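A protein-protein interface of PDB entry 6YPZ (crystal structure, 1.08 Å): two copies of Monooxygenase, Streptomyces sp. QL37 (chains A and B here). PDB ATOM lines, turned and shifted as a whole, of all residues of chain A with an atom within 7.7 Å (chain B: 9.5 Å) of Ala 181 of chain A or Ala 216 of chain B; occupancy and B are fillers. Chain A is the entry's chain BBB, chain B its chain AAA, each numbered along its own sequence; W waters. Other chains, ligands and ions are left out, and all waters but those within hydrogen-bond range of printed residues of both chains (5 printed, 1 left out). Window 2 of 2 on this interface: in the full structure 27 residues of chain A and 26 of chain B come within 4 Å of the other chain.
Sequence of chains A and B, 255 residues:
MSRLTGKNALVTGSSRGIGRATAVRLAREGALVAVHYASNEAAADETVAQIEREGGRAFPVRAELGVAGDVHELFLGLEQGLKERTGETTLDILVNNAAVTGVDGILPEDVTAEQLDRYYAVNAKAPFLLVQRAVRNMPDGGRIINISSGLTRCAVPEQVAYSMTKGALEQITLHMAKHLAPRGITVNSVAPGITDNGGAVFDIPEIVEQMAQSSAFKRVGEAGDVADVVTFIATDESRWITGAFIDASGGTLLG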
ATOM      1  N   ASP A 140     -26.275  -6.152  -6.704  1.00  0.00           N
ATOM      2  CA  ASP A 140     -24.911  -6.056  -6.260  1.00  0.00           C
ATOM      3  C   ASP A 140     -24.935  -5.490  -4.877  1.00  0.00           C
ATOM      4  O   ASP A 140     -25.764  -4.633  -4.433  1.00  0.00           O
ATOM      5  CB  ASP A 140     -24.088  -5.171  -7.213  1.00  0.00           C
ATOM      6  CG  ASP A 140     -23.681  -5.835  -8.507  1.00  0.00           C
ATOM      7  OD1 ASP A 140     -24.191  -6.837  -8.930  1.00  0.00           O
ATOM      8  OD2 ASP A 140     -22.763  -5.236  -9.108  1.00  0.00           O
ATOM      9  N   GLY A 141     -24.092  -6.044  -4.001  1.00  0.00           N
ATOM     10  CA  GLY A 141     -24.125  -5.601  -2.654  1.00  0.00           C
ATOM     11  C   GLY A 141     -24.983  -6.450  -1.687  1.00  0.00           C
ATOM     12  O   GLY A 141     -25.143  -6.148  -0.516  1.00  0.00           O
ATOM     13  N   HIS A 175     -16.917 -21.457  -1.557  1.00  0.00           N
ATOM     14  CA  HIS A 175     -16.802 -21.393  -3.012  1.00  0.00           C
ATOM     15  C   HIS A 175     -17.746 -20.348  -3.603  1.00  0.00           C
ATOM     16  O   HIS A 175     -17.376 -19.675  -4.581  1.00  0.00           O
ATOM     17  CB  HIS A 175     -17.030 -22.805  -3.596  1.00  0.00           C
ATOM     18  CG  HIS A 175     -15.995 -23.762  -3.145  1.00  0.00           C
ATOM     19  ND1 HIS A 175     -16.067 -24.627  -2.098  1.00  0.00           N
ATOM     20  CD2 HIS A 175     -14.736 -23.798  -3.637  1.00  0.00           C
ATOM     21  CE1 HIS A 175     -14.844 -25.211  -1.995  1.00  0.00           C
ATOM     22  NE2 HIS A 175     -14.052 -24.690  -2.924  1.00  0.00           N
ATOM     23  N   MET A 176     -18.911 -20.165  -3.011  1.00  0.00           N
ATOM     24  CA  MET A 176     -19.800 -19.127  -3.527  1.00  0.00           C
ATOM     25  C   MET A 176     -19.316 -17.739  -3.132  1.00  0.00           C
ATOM     26  O   MET A 176     -19.579 -16.790  -3.889  1.00  0.00           O
ATOM     27  CB  MET A 176     -21.233 -19.320  -3.051  1.00  0.00           C
ATOM     28  CG  MET A 176     -21.871 -20.595  -3.587  1.00  0.00           C
ATOM     29  SD  MET A 176     -21.876 -20.769  -5.354  1.00  0.00           S
ATOM     30  CE  MET A 176     -23.013 -19.470  -5.839  1.00  0.00           C
ATOM     31  N   ALA A 177     -18.582 -17.566  -2.043  1.00  0.00           N
ATOM     32  CA  ALA A 177     -18.011 -16.233  -1.775  1.00  0.00           C
ATOM     33  C   ALA A 177     -17.102 -15.834  -2.920  1.00  0.00           C
ATOM     34  O   ALA A 177     -17.132 -14.667  -3.371  1.00  0.00           O
ATOM     35  CB  ALA A 177     -17.242 -16.247  -0.458  1.00  0.00           C
ATOM     36  N   LYS A 178     -16.246 -16.748  -3.388  1.00  0.00           N
ATOM     37  CA  LYS A 178     -15.381 -16.385  -4.512  1.00  0.00           C
ATOM     38  C   LYS A 178     -16.213 -16.147  -5.775  1.00  0.00           C
ATOM     39  O   LYS A 178     -15.959 -15.175  -6.516  1.00  0.00           O
ATOM     40  CB  LYS A 178     -14.389 -17.518  -4.737  1.00  0.00           C
ATOM     41  CG  LYS A 178     -13.443 -17.298  -5.905  1.00  0.00           C
ATOM     42  CD  LYS A 178     -12.547 -16.181  -5.742  1.00  0.00           C
ATOM     43  CE  LYS A 178     -11.525 -16.112  -6.854  1.00  0.00           C
ATOM     44  NZ  LYS A 178     -10.610 -14.946  -6.712  1.00  0.00           N
ATOM     45  N   HIS A 179     -17.199 -16.993  -6.027  1.00  0.00           N
ATOM     46  CA  HIS A 179     -18.018 -16.849  -7.261  1.00  0.00           C
ATOM     47  C   HIS A 179     -18.729 -15.517  -7.305  1.00  0.00           C
ATOM     48  O   HIS A 179     -18.836 -14.940  -8.399  1.00  0.00           O
ATOM     49  CB  HIS A 179     -19.010 -17.969  -7.307  1.00  0.00           C
ATOM     50  CG  HIS A 179     -19.770 -18.024  -8.587  1.00  0.00           C
ATOM     51  ND1 HIS A 179     -19.161 -18.226  -9.779  1.00  0.00           N
ATOM     52  CD2 HIS A 179     -21.066 -17.804  -8.809  1.00  0.00           C
ATOM     53  CE1 HIS A 179     -20.186 -18.194 -10.699  1.00  0.00           C
ATOM     54  NE2 HIS A 179     -21.230 -17.951 -10.171  1.00  0.00           N
ATOM     55  N   LEU A 180     -19.271 -15.084  -6.186  1.00  0.00           N
ATOM     56  CA  LEU A 180     -20.188 -13.920  -6.165  1.00  0.00           C
ATOM     57  C   LEU A 180     -19.478 -12.622  -5.840  1.00  0.00           C
ATOM     58  O   LEU A 180     -20.055 -11.550  -5.939  1.00  0.00           O
ATOM     59  CB  LEU A 180     -21.302 -14.183  -5.167  1.00  0.00           C
ATOM     60  CG  LEU A 180     -22.242 -15.316  -5.570  1.00  0.00           C
ATOM     61  CD1 LEU A 180     -23.189 -15.616  -4.487  1.00  0.00           C
ATOM     62  CD2 LEU A 180     -22.999 -15.010  -6.876  1.00  0.00           C
ATOM     63  N   ALA A 181     -18.199 -12.676  -5.489  1.00  0.00           N
ATOM     64  CA  ALA A 181     -17.417 -11.500  -5.155  1.00  0.00           C
ATOM     65  C   ALA A 181     -17.463 -10.428  -6.254  1.00  0.00           C
ATOM     66  O   ALA A 181     -17.568  -9.233  -5.923  1.00  0.00           O
ATOM     67  CB  ALA A 181     -15.992 -11.827  -4.812  1.00  0.00           C
ATOM     68  N   PRO A 182     -17.413 -10.754  -7.562  1.00  0.00           N
ATOM     69  CA  PRO A 182     -17.489  -9.737  -8.608  1.00  0.00           C
ATOM     70  C   PRO A 182     -18.776  -8.932  -8.544  1.00  0.00           C
ATOM     71  O   PRO A 182     -18.813  -7.824  -9.111  1.00  0.00           O
ATOM     72  CB  PRO A 182     -17.346 -10.461  -9.944  1.00  0.00           C
ATOM     73  CG  PRO A 182     -16.622 -11.729  -9.528  1.00  0.00           C
ATOM     74  CD  PRO A 182     -17.153 -12.079  -8.154  1.00  0.00           C
ATOM     75  N   ARG A 183     -19.844  -9.482  -7.977  1.00  0.00           N
ATOM     76  CA  ARG A 183     -21.114  -8.758  -7.806  1.00  0.00           C
ATOM     77  C   ARG A 183     -21.159  -8.028  -6.474  1.00  0.00           C
ATOM     78  O   ARG A 183     -22.206  -7.409  -6.111  1.00  0.00           O
ATOM     79  CB  ARG A 183     -22.267  -9.747  -7.913  1.00  0.00           C
ATOM     80  CG  ARG A 183     -22.376 -10.321  -9.315  1.00  0.00           C
ATOM     81  CD  ARG A 183     -23.285 -11.566  -9.359  1.00  0.00           C
ATOM     82  NE  ARG A 183     -24.685 -11.212  -9.107  1.00  0.00           N
ATOM     83  CZ  ARG A 183     -25.758 -11.990  -9.287  1.00  0.00           C
ATOM     84  NH1 ARG A 183     -25.664 -13.223  -9.708  1.00  0.00           N
ATOM     85  NH2 ARG A 183     -26.943 -11.500  -8.983  1.00  0.00           N
ATOM     86  N   GLY A 184     -20.157  -8.093  -5.663  1.00  0.00           N
ATOM     87  CA  GLY A 184     -20.250  -7.453  -4.356  1.00  0.00           C
ATOM     88  C   GLY A 184     -21.206  -8.172  -3.441  1.00  0.00           C
ATOM     89  O   GLY A 184     -21.720  -7.508  -2.476  1.00  0.00           O
ATOM     90  N   ILE A 185     -21.588  -9.394  -3.683  1.00  0.00           N
ATOM     91  CA  ILE A 185     -22.435 -10.163  -2.790  1.00  0.00           C
ATOM     92  C   ILE A 185     -21.518 -10.913  -1.849  1.00  0.00           C
ATOM     93  O   ILE A 185     -20.690 -11.706  -2.358  1.00  0.00           O
ATOM     94  CB  ILE A 185     -23.346 -11.091  -3.591  1.00  0.00           C
ATOM     95  CG1 ILE A 185     -24.369 -10.291  -4.389  1.00  0.00           C
ATOM     96  CG2 ILE A 185     -24.034 -12.077  -2.652  1.00  0.00           C
ATOM     97  CD1 ILE A 185     -25.089 -11.071  -5.442  1.00  0.00           C
ATOM     98  N   THR A 186     -21.654 -10.774  -0.554  1.00  0.00           N
ATOM     99  CA  THR A 186     -20.853 -11.537   0.397  1.00  0.00           C
ATOM    100  C   THR A 186     -21.580 -12.794   0.768  1.00  0.00           C
ATOM    101  O   THR A 186     -22.806 -12.863   0.773  1.00  0.00           O
ATOM    102  CB  THR A 186     -20.430 -10.705   1.598  1.00  0.00           C
ATOM    103  OG1 THR A 186     -21.590 -10.499   2.404  1.00  0.00           O
ATOM    104  CG2 THR A 186     -19.775  -9.404   1.214  1.00  0.00           C
ATOM    105  N   VAL A 187     -20.795 -13.795   1.157  1.00  0.00           N
ATOM    106  CA  VAL A 187     -21.325 -15.108   1.551  1.00  0.00           C
ATOM    107  C   VAL A 187     -20.539 -15.519   2.793  1.00  0.00           C
ATOM    108  O   VAL A 187     -19.297 -15.664   2.681  1.00  0.00           O
ATOM    109  CB  VAL A 187     -21.219 -16.187   0.474  1.00  0.00           C
ATOM    110  CG1 VAL A 187     -21.959 -17.411   0.886  1.00  0.00           C
ATOM    111  CG2 VAL A 187     -21.685 -15.657  -0.898  1.00  0.00           C
ATOM    112  N   TRP A 240     -16.462  -6.049   4.070  1.00  0.00           N
ATOM    113  CA  TRP A 240     -15.113  -6.572   3.845  1.00  0.00           C
ATOM    114  C   TRP A 240     -14.941  -7.966   4.430  1.00  0.00           C
ATOM    115  O   TRP A 240     -13.814  -8.499   4.407  1.00  0.00           O
ATOM    116  CB  TRP A 240     -14.111  -5.523   4.384  1.00  0.00           C
ATOM    117  CG  TRP A 240     -12.816  -5.468   3.693  1.00  0.00           C
ATOM    118  CD1 TRP A 240     -11.590  -5.530   4.291  1.00  0.00           C
ATOM    119  CD2 TRP A 240     -12.595  -5.340   2.314  1.00  0.00           C
ATOM    120  NE1 TRP A 240     -10.623  -5.452   3.351  1.00  0.00           N
ATOM    121  CE2 TRP A 240     -11.175  -5.325   2.129  1.00  0.00           C
ATOM    122  CE3 TRP A 240     -13.378  -5.179   1.220  1.00  0.00           C
ATOM    123  CZ2 TRP A 240     -10.612  -5.261   0.875  1.00  0.00           C
ATOM    124  CZ3 TRP A 240     -12.804  -5.095  -0.060  1.00  0.00           C
ATOM    125  CH2 TRP A 240     -11.437  -5.099  -0.181  1.00  0.00           C
ATOM    126  N   THR A 242     -16.013 -11.732   3.725  1.00  0.00           N
ATOM    127  CA  THR A 242     -16.662 -12.689   2.821  1.00  0.00           C
ATOM    128  C   THR A 242     -15.901 -13.996   2.889  1.00  0.00           C
ATOM    129  O   THR A 242     -14.674 -14.016   3.100  1.00  0.00           O
ATOM    130  CB  THR A 242     -16.806 -12.182   1.392  1.00  0.00           C
ATOM    131  OG1 THR A 242     -17.811 -12.984   0.764  1.00  0.00           O
ATOM    132  CG2 THR A 242     -15.527 -12.186   0.617  1.00  0.00           C
ATOM    133  N   GLY B 193      -6.531  -7.635   5.300  1.00  0.00           N
ATOM    134  CA  GLY B 193      -5.710  -7.879   4.150  1.00  0.00           C
ATOM    135  C   GLY B 193      -4.982  -6.611   3.810  1.00  0.00           C
ATOM    136  O   GLY B 193      -4.773  -5.738   4.664  1.00  0.00           O
ATOM    137  N   MET B 211      -1.542  -5.181  -5.913  1.00  0.00           N
ATOM    138  CA  MET B 211      -2.011  -5.456  -4.536  1.00  0.00           C
ATOM    139  C   MET B 211      -3.492  -5.813  -4.608  1.00  0.00           C
ATOM    140  O   MET B 211      -3.902  -6.697  -3.842  1.00  0.00           O
ATOM    141  CB  MET B 211      -1.761  -4.205  -3.688  1.00  0.00           C
ATOM    142  CG  MET B 211      -0.316  -3.918  -3.452  1.00  0.00           C
ATOM    143  SD  MET B 211      -0.036  -2.581  -2.243  1.00  0.00           S
ATOM    144  CE  MET B 211      -0.605  -1.087  -3.002  1.00  0.00           C
ATOM    145  N   ALA B 212      -4.269  -5.070  -5.365  1.00  0.00           N
ATOM    146  CA  ALA B 212      -5.742  -5.281  -5.447  1.00  0.00           C
ATOM    147  C   ALA B 212      -6.056  -6.704  -5.875  1.00  0.00           C
ATOM    148  O   ALA B 212      -7.137  -7.279  -5.447  1.00  0.00           O
ATOM    149  CB  ALA B 212      -6.349  -4.289  -6.328  1.00  0.00           C
ATOM    150  N   GLN B 213      -5.186  -7.434  -6.567  1.00  0.00           N
ATOM    151  CA  GLN B 213      -5.567  -8.771  -7.055  1.00  0.00           C
ATOM    152  C   GLN B 213      -5.666  -9.776  -5.907  1.00  0.00           C
ATOM    153  O   GLN B 213      -6.248 -10.801  -6.125  1.00  0.00           O
ATOM    154  CB  GLN B 213      -4.566  -9.252  -8.129  1.00  0.00           C
ATOM    155  CG  GLN B 213      -4.335  -8.288  -9.294  1.00  0.00           C
ATOM    156  CD  GLN B 213      -5.626  -7.820  -9.889  1.00  0.00           C
ATOM    157  OE1 GLN B 213      -6.425  -8.667 -10.277  1.00  0.00           O
ATOM    158  NE2 GLN B 213      -5.935  -6.534  -9.895  1.00  0.00           N
ATOM    159  N   SER B 214      -5.087  -9.474  -4.733  1.00  0.00           N
ATOM    160  CA  SER B 214      -5.122 -10.377  -3.582  1.00  0.00           C
ATOM    161  C   SER B 214      -6.558 -10.527  -3.047  1.00  0.00           C
ATOM    162  O   SER B 214      -6.848 -11.565  -2.463  1.00  0.00           O
ATOM    163  CB  SER B 214      -4.164  -9.980  -2.506  1.00  0.00           C
ATOM    164  OG  SER B 214      -4.435  -8.696  -2.003  1.00  0.00           O
ATOM    165  N   SER B 215      -7.333  -9.488  -3.175  1.00  0.00           N
ATOM    166  CA  SER B 215      -8.739  -9.523  -2.678  1.00  0.00           C
ATOM    167  C   SER B 215      -9.651 -10.147  -3.712  1.00  0.00           C
ATOM    168  O   SER B 215      -9.552  -9.902  -4.934  1.00  0.00           O
ATOM    169  CB  SER B 215      -9.233  -8.146  -2.358  1.00  0.00           C
ATOM    170  OG  SER B 215     -10.642  -8.070  -2.269  1.00  0.00           O
ATOM    171  N   ALA B 216     -10.653 -10.897  -3.272  1.00  0.00           N
ATOM    172  CA  ALA B 216     -11.672 -11.437  -4.177  1.00  0.00           C
ATOM    173  C   ALA B 216     -12.472 -10.305  -4.855  1.00  0.00           C
ATOM    174  O   ALA B 216     -13.045 -10.488  -5.947  1.00  0.00           O
ATOM    175  CB  ALA B 216     -12.643 -12.302  -3.412  1.00  0.00           C
ATOM    176  N   PHE B 217     -12.489  -9.141  -4.247  1.00  0.00           N
ATOM    177  CA  PHE B 217     -13.168  -7.935  -4.740  1.00  0.00           C
ATOM    178  C   PHE B 217     -12.280  -7.142  -5.700  1.00  0.00           C
ATOM    179  O   PHE B 217     -12.778  -6.153  -6.264  1.00  0.00           O
ATOM    180  CB  PHE B 217     -13.698  -7.057  -3.610  1.00  0.00           C
ATOM    181  CG  PHE B 217     -14.673  -7.795  -2.730  1.00  0.00           C
ATOM    182  CD1 PHE B 217     -15.875  -8.294  -3.194  1.00  0.00           C
ATOM    183  CD2 PHE B 217     -14.389  -7.951  -1.370  1.00  0.00           C
ATOM    184  CE1 PHE B 217     -16.709  -8.991  -2.360  1.00  0.00           C
ATOM    185  CE2 PHE B 217     -15.286  -8.620  -0.557  1.00  0.00           C
ATOM    186  CZ  PHE B 217     -16.427  -9.129  -1.038  1.00  0.00           C
ATOM    187  N   LYS B 218     -11.043  -7.529  -5.822  1.00  0.00           N
ATOM    188  CA  LYS B 218     -10.096  -6.904  -6.789  1.00  0.00           C
ATOM    189  C   LYS B 218      -9.987  -5.415  -6.500  1.00  0.00           C
ATOM    190  O   LYS B 218      -9.841  -4.582  -7.438  1.00  0.00           O
ATOM    191  CB  LYS B 218     -10.481  -7.189  -8.233  1.00  0.00           C
ATOM    192  CG  LYS B 218     -10.550  -8.685  -8.503  1.00  0.00           C
ATOM    193  CD  LYS B 218      -9.273  -9.384  -8.309  1.00  0.00           C
ATOM    194  CE  LYS B 218      -9.450 -10.895  -8.282  1.00  0.00           C
ATOM    195  NZ  LYS B 218      -8.152 -11.620  -8.358  1.00  0.00           N
ATOM    196  N   ARG B 219      -9.909  -5.044  -5.213  1.00  0.00           N
ATOM    197  CA  ARG B 219      -9.565  -3.684  -4.761  1.00  0.00           C
ATOM    198  C   ARG B 219      -8.793  -3.876  -3.483  1.00  0.00           C
ATOM    199  O   ARG B 219      -8.906  -4.892  -2.798  1.00  0.00           O
ATOM    200  CB  ARG B 219     -10.725  -2.747  -4.550  1.00  0.00           C
ATOM    201  CG  ARG B 219     -11.674  -3.153  -3.422  1.00  0.00           C
ATOM    202  CD  ARG B 219     -12.739  -2.074  -3.220  1.00  0.00           C
ATOM    203  NE  ARG B 219     -13.730  -2.279  -2.178  1.00  0.00           N
ATOM    204  CZ  ARG B 219     -13.560  -1.943  -0.890  1.00  0.00           C
ATOM    205  NH1 ARG B 219     -12.390  -1.461  -0.473  1.00  0.00           N
ATOM    206  NH2 ARG B 219     -14.585  -2.092  -0.074  1.00  0.00           N
ATOM    207  N   VAL B 220      -7.940  -2.922  -3.172  1.00  0.00           N
ATOM    208  CA  VAL B 220      -7.339  -2.868  -1.839  1.00  0.00           C
ATOM    209  C   VAL B 220      -8.378  -2.432  -0.826  1.00  0.00           C
ATOM    210  O   VAL B 220      -9.330  -1.756  -1.143  1.00  0.00           O
ATOM    211  CB  VAL B 220      -6.056  -2.028  -1.732  1.00  0.00           C
ATOM    212  CG1 VAL B 220      -4.957  -2.563  -2.676  1.00  0.00           C
ATOM    213  CG2 VAL B 220      -6.324  -0.575  -1.836  1.00  0.00           C
ATOM    214  N   GLY B 221      -8.208  -2.817   0.395  1.00  0.00           N
ATOM    215  CA  GLY B 221      -9.084  -2.383   1.466  1.00  0.00           C
ATOM    216  C   GLY B 221      -8.922  -0.922   1.764  1.00  0.00           C
ATOM    217  O   GLY B 221      -7.810  -0.370   1.627  1.00  0.00           O
ATOM    218  N   ASP B 247     -12.181 -12.543   9.845  1.00  0.00           N
ATOM    219  CA  ASP B 247     -11.551 -12.200   8.577  1.00  0.00           C
ATOM    220  C   ASP B 247     -12.082 -10.874   8.049  1.00  0.00           C
ATOM    221  O   ASP B 247     -13.299 -10.787   7.698  1.00  0.00           O
ATOM    222  CB  ASP B 247     -11.847 -13.341   7.603  1.00  0.00           C
ATOM    223  CG  ASP B 247     -11.250 -13.178   6.264  1.00  0.00           C
ATOM    224  OD1 ASP B 247     -11.057 -12.062   5.755  1.00  0.00           O
ATOM    225  OD2 ASP B 247     -11.047 -14.276   5.595  1.00  0.00           O
ATOM    226  N   SER B 249     -10.567  -9.143   5.440  1.00  0.00           N
ATOM    227  CA  SER B 249      -9.535  -9.091   4.372  1.00  0.00           C
ATOM    228  C   SER B 249     -10.132  -8.876   3.010  1.00  0.00           C
ATOM    229  O   SER B 249      -9.362  -8.960   2.015  1.00  0.00           O
ATOM    230  CB  SER B 249      -8.673 -10.328   4.391  1.00  0.00           C
ATOM    231  OG  SER B 249      -9.369 -11.433   3.804  1.00  0.00           O
ATOM    232  N   GLY B 250     -11.411  -8.675   2.853  1.00  0.00           N
ATOM    233  CA  GLY B 250     -11.961  -8.571   1.505  1.00  0.00           C
ATOM    234  C   GLY B 250     -11.792  -9.872   0.727  1.00  0.00           C
ATOM    235  O   GLY B 250     -11.519  -9.836  -0.510  1.00  0.00           O
ATOM    236  N   GLY B 251     -11.942 -10.998   1.361  1.00  0.00           N
ATOM    237  CA  GLY B 251     -11.858 -12.244   0.605  1.00  0.00           C
ATOM    238  C   GLY B 251     -10.456 -12.589   0.187  1.00  0.00           C
ATOM    239  O   GLY B 251     -10.295 -13.240  -0.873  1.00  0.00           O
ATOM    240  N   THR B 252      -9.462 -12.185   0.870  1.00  0.00           N
ATOM    241  CA  THR B 252      -8.062 -12.547   0.509  1.00  0.00           C
ATOM    242  C   THR B 252      -7.802 -13.998   0.875  1.00  0.00           C
ATOM    243  O   THR B 252      -6.880 -14.573   0.205  1.00  0.00           O
ATOM    244  CB  THR B 252      -7.084 -11.639   1.252  1.00  0.00           C
ATOM    245  OG1 THR B 252      -7.332 -10.276   0.921  1.00  0.00           O
ATOM    246  CG2 THR B 252      -5.616 -11.955   1.043  1.00  0.00           C
ATOM    247  N   LEU B 253      -8.446 -14.562   1.839  1.00  0.00           N
ATOM    248  CA  LEU B 253      -8.168 -15.891   2.532  1.00  0.00           C
ATOM    249  C   LEU B 253      -9.113 -16.920   1.937  1.00  0.00           C
ATOM    250  O   LEU B 253      -9.657 -17.701   2.849  1.00  0.00           O
ATOM    251  CB  LEU B 253      -8.382 -15.702   4.035  1.00  0.00           C
ATOM    252  CG  LEU B 253      -7.478 -14.639   4.679  1.00  0.00           C
ATOM    253  CD1 LEU B 253      -7.633 -14.662   6.218  1.00  0.00           C
ATOM    254  CD2 LEU B 253      -6.058 -14.788   4.263  1.00  0.00           C
ATOM    255  N   LEU B 254      -9.411 -16.814   0.657  1.00  0.00           N
ATOM    256  CA  LEU B 254     -10.221 -17.834  -0.065  1.00  0.00           C
ATOM    257  C   LEU B 254      -9.297 -18.921  -0.582  1.00  0.00           C
ATOM    258  O   LEU B 254      -9.755 -20.077  -0.829  1.00  0.00           O
ATOM    259  CB  LEU B 254     -11.134 -17.123  -1.107  1.00  0.00           C
ATOM    260  CG  LEU B 254     -12.267 -16.289  -0.457  1.00  0.00           C
ATOM    261  CD1 LEU B 254     -13.184 -15.535  -1.375  1.00  0.00           C
ATOM    262  CD2 LEU B 254     -13.111 -17.302   0.236  1.00  0.00           C
HETATM  263  O   HOH W   1      -8.417 -12.923  -5.457  1.00  0.00           O
HETATM  264  O   HOH W   2      -9.247 -14.754  -9.093  1.00  0.00           O
HETATM  265  O   HOH W   3      -7.833  -5.408   3.800  1.00  0.00           O
HETATM  266  O   HOH W   4     -11.454 -14.298   2.965  1.00  0.00           O
HETATM  267  O   HOH W   5     -12.484 -12.828  -7.161  1.00  0.00           O
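CD1 of Leu 254 of chain B touches N of Lys 178 of chain A, 3.9 Å away. Ala 181 of chain A touches Ala 216 of chain B (CB to O, 3.4 Å). Ala 181 of chain A touches Phe 217 of chain B (O to CD1, 3.3 Å). Trp 240 of chain A touches Ser 215 of chain B. Phe 217 of chain B touches Trp 240 of chain A. Trp 240 of chain A touches Arg 219 of chain B (CZ3 to CZ, 3.3 Å). Trp 240 of chain A touches Val 220 of chain B (CZ2 to C, 3.99 Å). Trp 240 of chain A touches Gly 221 of chain B. Thr 242 of chain A touches Phe 217 of chain B (CG2 to CZ, 3.6 Å). Thr 242 of chain A touches Gly 251 of chain B.
Of the 19 printed residues of chain B, 10 touch a printed residue of chain A. Hydrophobic or aromatic side chains of chain B that line the printed part of chain A: Ala 216, Phe 217 and Leu 254. Among the printed residues, 12 pairs touch across the chains. Among the printed residues, no Asp or Glu carboxylate lies within 4 Å of a Lys or Arg side-chain nitrogen of the other chain.
The backbone NH of Ala 216 of chain B sits at hydrogen-bond distance from the backbone carbonyl oxygen of Gly 251 of chain B (3.4 Å). OD1 of Asp 247 of chain B lies within hydrogen-bond range of OG of Ser 249 of chain B. OG1 of Thr 242 of chain A lies within hydrogen-bond range of N of Val 187 of chain A (3.1 Å). The backbone NH (N) of Ala 216 of chain B is in hydrogen-bond range of the backbone carbonyl oxygen (O) of Gly 250 of chain B, at 3.1 Å. OG of Ser 215 of chain B is in hydrogen-bond range of O of Gly 250 of chain B (2.6 Å). The side-chain hydroxyl (OG1) of Thr 252 of chain B lies within hydrogen-bond range of the backbone carbonyl oxygen (O) of Ser 249 of chain B (2.7 Å).
Of chain B, only Ala 216 and Phe 217 come within 4 Å of Ala 181 of chain A. No residue of chain B comes within 4 Å of Pro 182 of chain A. Of the printed residues of chain B, Thr 242 of chain A touches Phe 217 and Gly 251. Of chain A, only Trp 240 comes within 4 Å of Ser 215 of chain B. Ala 216 of chain B touches just one residue of chain A: Ala 181. Of the printed residues of chain A, Gly 221 of chain B touches Trp 240 (3.3 Å). The nearest residue of chain A that does not touch Ala 216 of chain B is Lys 178 of chain A (4.5 Å).
Water W4 lies within hydrogen-bond range of the side-chain carboxylate (OD2) of Asp 247 of chain B (2.7 Å), the backbone NH (N) of Leu 253 of chain B (3.2 Å) and the backbone carbonyl oxygen (O) of Thr 242 of chain A (3.2 Å). Water W5 bridges O of Ala 216 of chain B (2.7 Å) and NZ of Lys 178 of chain A (2.9 Å). Water W2 lies within hydrogen-bond range of the side-chain amino group (NZ) of Lys 178 of chain A (2.8 Å) and the side-chain amino group (NZ) of Lys 218 of chain B (3.4 Å). Water W3 lies within hydrogen-bond range of NE1 of Trp 240 of chain A (2.8 Å) and N of Gly 193 of chain B (3.0 Å). Water W1 lies within hydrogen-bond range of the backbone carbonyl oxygen (O) of Gln 213 of chain B (3.1 Å), the side-chain amino group (NZ) of Lys 218 of chain B (3.2 Å), the side-chain amino group (NZ) of Lys 178 of chain A (3.2 Å) and the backbone carbonyl oxygen (O) of Ser 215 of chain B (3.3 Å).
No position is printed for both chains. Of the 12 pairs that touch across the chains among the printed residues, none has its exchanged pair printed and touching as well.
The backbone carbonyl oxygen of Trp 240 of chain A sits at hydrogen-bond distance from the backbone NH of Gly 250 of chain B, 2.9 Å away. N of Ser 249 of chain B sits at hydrogen-bond distance from O of Trp 240 of chain A (3.5 Å).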
